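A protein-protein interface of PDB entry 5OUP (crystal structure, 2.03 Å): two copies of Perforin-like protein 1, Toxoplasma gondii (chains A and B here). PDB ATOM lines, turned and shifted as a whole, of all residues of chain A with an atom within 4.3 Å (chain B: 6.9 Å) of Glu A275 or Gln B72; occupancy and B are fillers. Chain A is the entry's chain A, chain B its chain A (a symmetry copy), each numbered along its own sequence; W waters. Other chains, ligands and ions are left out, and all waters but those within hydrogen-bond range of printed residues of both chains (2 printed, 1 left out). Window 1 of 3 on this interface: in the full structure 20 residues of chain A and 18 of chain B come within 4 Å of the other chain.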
ATOM      1  N   THR A 218       8.232  27.129 -29.282  1.00  0.00           N
ATOM      2  CA  THR A 218       9.290  26.153 -29.494  1.00  0.00           C
ATOM      3  C   THR A 218       9.681  25.534 -28.162  1.00  0.00           C
ATOM      4  O   THR A 218       9.891  26.251 -27.174  1.00  0.00           O
ATOM      5  CB  THR A 218      10.513  26.786 -30.168  1.00  0.00           C
ATOM      6  OG1 THR A 218      11.090  27.763 -29.297  1.00  0.00           O
ATOM      7  CG2 THR A 218      10.120  27.455 -31.471  1.00  0.00           C
ATOM      8  N   TYR A 219       9.769  24.209 -28.135  1.00  0.00           N
ATOM      9  CA  TYR A 219      10.249  23.477 -26.972  1.00  0.00           C
ATOM     10  C   TYR A 219      11.645  22.949 -27.261  1.00  0.00           C
ATOM     11  O   TYR A 219      11.864  22.287 -28.280  1.00  0.00           O
ATOM     12  CB  TYR A 219       9.314  22.318 -26.617  1.00  0.00           C
ATOM     13  CG  TYR A 219       7.868  22.715 -26.481  1.00  0.00           C
ATOM     14  CD1 TYR A 219       7.418  23.400 -25.363  1.00  0.00           C
ATOM     15  CD2 TYR A 219       6.947  22.398 -27.471  1.00  0.00           C
ATOM     16  CE1 TYR A 219       6.090  23.768 -25.235  1.00  0.00           C
ATOM     17  CE2 TYR A 219       5.619  22.761 -27.354  1.00  0.00           C
ATOM     18  CZ  TYR A 219       5.195  23.446 -26.234  1.00  0.00           C
ATOM     19  OH  TYR A 219       3.873  23.806 -26.113  1.00  0.00           O
ATOM     20  N   GLN A 220      12.584  23.254 -26.376  1.00  0.00           N
ATOM     21  CA  GLN A 220      13.919  22.671 -26.422  1.00  0.00           C
ATOM     22  C   GLN A 220      14.004  21.652 -25.295  1.00  0.00           C
ATOM     23  O   GLN A 220      13.968  22.014 -24.113  1.00  0.00           O
ATOM     24  CB  GLN A 220      14.992  23.751 -26.322  1.00  0.00           C
ATOM     25  CG  GLN A 220      15.086  24.548 -27.614  1.00  0.00           C
ATOM     26  CD  GLN A 220      16.021  25.733 -27.533  1.00  0.00           C
ATOM     27  OE1 GLN A 220      16.777  25.887 -26.573  1.00  0.00           O
ATOM     28  NE2 GLN A 220      15.971  26.583 -28.551  1.00  0.00           N
ATOM     29  N   LYS A 274      12.949  20.629 -20.163  1.00  0.00           N
ATOM     30  CA  LYS A 274      12.243  21.278 -21.261  1.00  0.00           C
ATOM     31  C   LYS A 274      12.158  22.773 -21.006  1.00  0.00           C
ATOM     32  O   LYS A 274      11.699  23.196 -19.942  1.00  0.00           O
ATOM     33  CB  LYS A 274      10.836  20.700 -21.443  1.00  0.00           C
ATOM     34  CG  LYS A 274      10.053  21.349 -22.578  1.00  0.00           C
ATOM     35  CD  LYS A 274       8.740  20.627 -22.834  1.00  0.00           C
ATOM     36  CE  LYS A 274       7.747  20.858 -21.708  1.00  0.00           C
ATOM     37  NZ  LYS A 274       7.322  22.281 -21.641  1.00  0.00           N
ATOM     38  N   GLU A 275      12.597  23.567 -21.978  1.00  0.00           N
ATOM     39  CA  GLU A 275      12.451  25.014 -21.953  1.00  0.00           C
ATOM     40  C   GLU A 275      11.493  25.435 -23.059  1.00  0.00           C
ATOM     41  O   GLU A 275      11.516  24.869 -24.155  1.00  0.00           O
ATOM     42  CB  GLU A 275      13.803  25.715 -22.130  1.00  0.00           C
ATOM     43  CG  GLU A 275      13.711  27.235 -22.206  1.00  0.00           C
ATOM     44  CD  GLU A 275      15.043  27.899 -22.519  1.00  0.00           C
ATOM     45  OE1 GLU A 275      15.149  29.130 -22.332  1.00  0.00           O
ATOM     46  OE2 GLU A 275      15.980  27.195 -22.952  1.00  0.00           O
ATOM     47  N   THR A 276      10.646  26.420 -22.770  1.00  0.00           N
ATOM     48  CA  THR A 276       9.692  26.939 -23.742  1.00  0.00           C
ATOM     49  C   THR A 276      10.121  28.323 -24.203  1.00  0.00           C
ATOM     50  O   THR A 276      10.407  29.197 -23.379  1.00  0.00           O
ATOM     51  CB  THR A 276       8.277  27.015 -23.165  1.00  0.00           C
ATOM     52  OG1 THR A 276       7.875  25.717 -22.713  1.00  0.00           O
ATOM     53  CG2 THR A 276       7.306  27.494 -24.244  1.00  0.00           C
ATOM     54  N   LEU A 277      10.148  28.520 -25.517  1.00  0.00           N
ATOM     55  CA  LEU A 277      10.480  29.801 -26.125  1.00  0.00           C
ATOM     56  C   LEU A 277       9.328  30.204 -27.036  1.00  0.00           C
ATOM     57  O   LEU A 277       8.883  29.405 -27.866  1.00  0.00           O
ATOM     58  CB  LEU A 277      11.793  29.718 -26.910  1.00  0.00           C
ATOM     59  CG  LEU A 277      12.995  29.050 -26.230  1.00  0.00           C
ATOM     60  CD1 LEU A 277      13.035  27.544 -26.485  1.00  0.00           C
ATOM     61  CD2 LEU A 277      14.283  29.697 -26.690  1.00  0.00           C
ATOM     62  N   PRO A 284       2.641  34.396 -22.329  1.00  0.00           N
ATOM     63  CA  PRO A 284       1.846  33.271 -21.816  1.00  0.00           C
ATOM     64  C   PRO A 284       2.173  32.934 -20.369  1.00  0.00           C
ATOM     65  O   PRO A 284       3.344  32.816 -19.999  1.00  0.00           O
ATOM     66  CB  PRO A 284       2.225  32.128 -22.766  1.00  0.00           C
ATOM     67  CG  PRO A 284       3.639  32.430 -23.142  1.00  0.00           C
ATOM     68  CD  PRO A 284       3.796  33.941 -23.125  1.00  0.00           C
ATOM     69  N   GLY A 285       1.138  32.772 -19.545  1.00  0.00           N
ATOM     70  CA  GLY A 285       1.366  32.548 -18.127  1.00  0.00           C
ATOM     71  C   GLY A 285       1.915  31.167 -17.819  1.00  0.00           C
ATOM     72  O   GLY A 285       2.852  31.024 -17.028  1.00  0.00           O
ATOM     73  N   GLN A 286       1.345  30.133 -18.434  1.00  0.00           N
ATOM     74  CA  GLN A 286       1.732  28.759 -18.140  1.00  0.00           C
ATOM     75  C   GLN A 286       1.666  27.934 -19.413  1.00  0.00           C
ATOM     76  O   GLN A 286       0.590  27.774 -19.997  1.00  0.00           O
ATOM     77  CB  GLN A 286       0.831  28.152 -17.061  1.00  0.00           C
ATOM     78  CG  GLN A 286       1.365  26.862 -16.479  1.00  0.00           C
ATOM     79  CD  GLN A 286       2.769  27.020 -15.927  1.00  0.00           C
ATOM     80  OE1 GLN A 286       3.114  28.058 -15.359  1.00  0.00           O
ATOM     81  NE2 GLN A 286       3.590  25.990 -16.100  1.00  0.00           N
ATOM     82  N   VAL A 287       2.816  27.405 -19.838  1.00  0.00           N
ATOM     83  CA  VAL A 287       2.844  26.558 -21.024  1.00  0.00           C
ATOM     84  C   VAL A 287       2.249  25.189 -20.725  1.00  0.00           C
ATOM     85  O   VAL A 287       1.680  24.543 -21.616  1.00  0.00           O
ATOM     86  CB  VAL A 287       4.285  26.455 -21.553  1.00  0.00           C
ATOM     87  CG1 VAL A 287       4.779  27.827 -21.954  1.00  0.00           C
ATOM     88  CG2 VAL A 287       5.200  25.854 -20.490  1.00  0.00           C
ATOM     89  N   CYS B  70       7.406  35.525 -17.582  1.00  0.00           N
ATOM     90  CA  CYS B  70       8.220  34.514 -16.931  1.00  0.00           C
ATOM     91  C   CYS B  70       8.804  33.587 -17.982  1.00  0.00           C
ATOM     92  O   CYS B  70       8.115  33.167 -18.916  1.00  0.00           O
ATOM     93  CB  CYS B  70       7.412  33.710 -15.901  1.00  0.00           C
ATOM     94  SG  CYS B  70       5.912  32.921 -16.529  1.00  0.00           S
ATOM     95  N   ARG B  71      10.097  33.321 -17.834  1.00  0.00           N
ATOM     96  CA  ARG B  71      10.820  32.348 -18.639  1.00  0.00           C
ATOM     97  C   ARG B  71      10.576  30.974 -18.030  1.00  0.00           C
ATOM     98  O   ARG B  71      11.028  30.694 -16.914  1.00  0.00           O
ATOM     99  CB  ARG B  71      12.305  32.700 -18.657  1.00  0.00           C
ATOM    100  CG  ARG B  71      13.160  31.789 -19.501  1.00  0.00           C
ATOM    101  CD  ARG B  71      14.640  32.148 -19.384  1.00  0.00           C
ATOM    102  NE  ARG B  71      15.457  31.422 -20.355  1.00  0.00           N
ATOM    103  CZ  ARG B  71      16.784  31.496 -20.421  1.00  0.00           C
ATOM    104  NH1 ARG B  71      17.450  32.263 -19.569  1.00  0.00           N
ATOM    105  NH2 ARG B  71      17.444  30.800 -21.339  1.00  0.00           N
ATOM    106  N   GLN B  72       9.860  30.119 -18.750  1.00  0.00           N
ATOM    107  CA  GLN B  72       9.336  28.880 -18.194  1.00  0.00           C
ATOM    108  C   GLN B  72      10.187  27.695 -18.626  1.00  0.00           C
ATOM    109  O   GLN B  72      10.524  27.559 -19.807  1.00  0.00           O
ATOM    110  CB  GLN B  72       7.884  28.674 -18.622  1.00  0.00           C
ATOM    111  CG  GLN B  72       7.006  29.885 -18.352  1.00  0.00           C
ATOM    112  CD  GLN B  72       5.547  29.522 -18.180  1.00  0.00           C
ATOM    113  OE1 GLN B  72       4.860  29.195 -19.145  1.00  0.00           O
ATOM    114  NE2 GLN B  72       5.067  29.579 -16.943  1.00  0.00           N
ATOM    115  N   SER B  73      10.519  26.839 -17.665  1.00  0.00           N
ATOM    116  CA  SER B  73      11.212  25.593 -17.940  1.00  0.00           C
ATOM    117  C   SER B  73      10.763  24.562 -16.917  1.00  0.00           C
ATOM    118  O   SER B  73      10.386  24.903 -15.792  1.00  0.00           O
ATOM    119  CB  SER B  73      12.737  25.767 -17.907  1.00  0.00           C
ATOM    120  OG  SER B  73      13.181  26.161 -16.623  1.00  0.00           O
ATOM    121  N   GLU B  74      10.788  23.297 -17.323  1.00  0.00           N
ATOM    122  CA  GLU B  74      10.356  22.195 -16.477  1.00  0.00           C
ATOM    123  C   GLU B  74      11.350  21.053 -16.589  1.00  0.00           C
ATOM    124  O   GLU B  74      11.916  20.812 -17.660  1.00  0.00           O
ATOM    125  CB  GLU B  74       8.955  21.696 -16.862  1.00  0.00           C
ATOM    126  CG  GLU B  74       7.822  22.674 -16.585  1.00  0.00           C
ATOM    127  CD  GLU B  74       7.305  23.343 -17.843  1.00  0.00           C
ATOM    128  OE1 GLU B  74       7.569  24.551 -18.031  1.00  0.00           O
ATOM    129  OE2 GLU B  74       6.639  22.659 -18.649  1.00  0.00           O
ATOM    130  N   ASN B 131       9.303  23.099 -11.698  1.00  0.00           N
ATOM    131  CA  ASN B 131       8.666  24.075 -12.580  1.00  0.00           C
ATOM    132  C   ASN B 131       9.259  25.447 -12.287  1.00  0.00           C
ATOM    133  O   ASN B 131       8.975  26.035 -11.239  1.00  0.00           O
ATOM    134  CB  ASN B 131       7.149  24.085 -12.393  1.00  0.00           C
ATOM    135  CG  ASN B 131       6.524  22.730 -12.656  1.00  0.00           C
ATOM    136  OD1 ASN B 131       6.170  22.406 -13.788  1.00  0.00           O
ATOM    137  ND2 ASN B 131       6.393  21.928 -11.606  1.00  0.00           N
ATOM    138  N   TYR B 132      10.071  25.957 -13.215  1.00  0.00           N
ATOM    139  CA  TYR B 132      10.746  27.240 -13.045  1.00  0.00           C
ATOM    140  C   TYR B 132       9.910  28.378 -13.614  1.00  0.00           C
ATOM    141  O   TYR B 132       9.384  28.286 -14.727  1.00  0.00           O
ATOM    142  CB  TYR B 132      12.106  27.250 -13.742  1.00  0.00           C
ATOM    143  CG  TYR B 132      13.142  26.277 -13.230  1.00  0.00           C
ATOM    144  CD1 TYR B 132      13.127  24.943 -13.625  1.00  0.00           C
ATOM    145  CD2 TYR B 132      14.169  26.703 -12.398  1.00  0.00           C
ATOM    146  CE1 TYR B 132      14.091  24.058 -13.182  1.00  0.00           C
ATOM    147  CE2 TYR B 132      15.139  25.825 -11.952  1.00  0.00           C
ATOM    148  CZ  TYR B 132      15.095  24.505 -12.347  1.00  0.00           C
ATOM    149  OH  TYR B 132      16.061  23.631 -11.907  1.00  0.00           O
ATOM    150  N   CYS B 133       9.825  29.472 -12.854  1.00  0.00           N
ATOM    151  CA  CYS B 133       9.147  30.704 -13.269  1.00  0.00           C
ATOM    152  C   CYS B 133      10.146  31.854 -13.103  1.00  0.00           C
ATOM    153  O   CYS B 133      10.080  32.619 -12.139  1.00  0.00           O
ATOM    154  CB  CYS B 133       7.871  30.921 -12.452  1.00  0.00           C
ATOM    155  SG  CYS B 133       6.983  32.447 -12.813  1.00  0.00           S
ATOM    156  N   MET B 134      11.072  31.975 -14.053  1.00  0.00           N
ATOM    157  CA  MET B 134      12.174  32.925 -13.948  1.00  0.00           C
ATOM    158  C   MET B 134      11.756  34.301 -14.454  1.00  0.00           C
ATOM    159  O   MET B 134      11.168  34.424 -15.534  1.00  0.00           O
ATOM    160  CB  MET B 134      13.387  32.425 -14.731  1.00  0.00           C
ATOM    161  CG  MET B 134      14.052  31.203 -14.124  1.00  0.00           C
ATOM    162  SD  MET B 134      15.359  30.556 -15.182  1.00  0.00           S
ATOM    163  CE  MET B 134      14.388  29.863 -16.519  1.00  0.00           C
HETATM  164  O   HOH W   1       8.709  24.608 -20.338  1.00  0.00           O
HETATM  165  O   HOH W   2      17.687  29.355 -24.244  1.00  0.00           O
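The side-chain amino group (NZ) of Lys A274 lies within salt-bridge range of the side-chain carboxylate (OE2) of Glu B74. NH2 of Arg B71 lies within salt-bridge range of OE1 of Glu A275, 3.0 Å away. N of Thr A276 lies within hydrogen-bond range of O of Gln B72 (3.2 Å). The backbone carbonyl oxygen (O) of Gly A285 lies within hydrogen-bond range of the side-chain sulfur (SG) of Cys B70 (3.6 Å). O of Gly A285 sits at hydrogen-bond distance from NE2 of Gln B72 (2.6 Å). The side-chain amide nitrogen of Gln B72 sits at hydrogen-bond distance from the side-chain amide oxygen of Gln A286 (2.9 Å). The backbone NH (N) of Val A287 is in hydrogen-bond range of the side-chain amide oxygen (OE1) of Gln B72, at 2.8 Å.
O of Glu A275 lies within hydrogen-bond range of N of Gln A220, at 2.9 Å. NE2 of Gln B72 lies within hydrogen-bond range of SG of Cys B70, at 3.5 Å. The backbone NH (N) of Arg B71 lies within hydrogen-bond range of the backbone carbonyl oxygen (O) of Met B134, at 2.8 Å. O of Ser B73 sits at hydrogen-bond distance from N of Tyr B132 (2.8 Å).
Among the printed residues, pairs that only touch across the chains: Lys A274 with Ser B73, Val A287 with Glu B74 and Glu A275 with Gln B72.
Glu A275 touches just these residues of chain B: Arg B71 (3.0 Å) and Gln B72 (3.8 Å). Printed residues of chain A within 4 Å of Gln B72: Glu A275, Thr A276, Gly A285, Gln A286 and Val A287. Printed residues of chain B within 4 Å of Gly A285: Cys B70 (3.6 Å) and Gln B72 (2.6 Å). Printed residues of chain B within 4 Å of Thr A276: Gln B72. Of the printed residues of chain A, Ser B73 touches Lys A274. Printed residues of chain A within 4 Å of Arg B71: Glu A275 (3.0 Å). Printed residues of chain B within 4 Å of Gln A286: Gln B72 (2.9 Å). Pro A284 touches none of the printed residues of chain B. Tyr B132 touches none of the printed residues of chain A.
Printed residues of chain B that touch a printed residue of chain A: Cys B70, Arg B71, Gln B72, Ser B73 and Glu B74. Along chain B the printed residues that touch a printed residue of chain A span positions 70 to 74. Of the 11 printed residues of chain A, 6 touch a printed residue of chain B. Among the printed residues, 10 pairs touch across the chains.
No position is printed for both chains.
Water W1 lies within hydrogen-bond range of OE1 of Glu B74 (2.6 Å), OG1 of Thr A276 (2.8 Å) and NZ of Lys A274 (3.0 Å). Water W2 lies within hydrogen-bond range of the side-chain carboxylate (OE2) of Glu A275 and the guanidinium group (NH2) of Arg B71.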
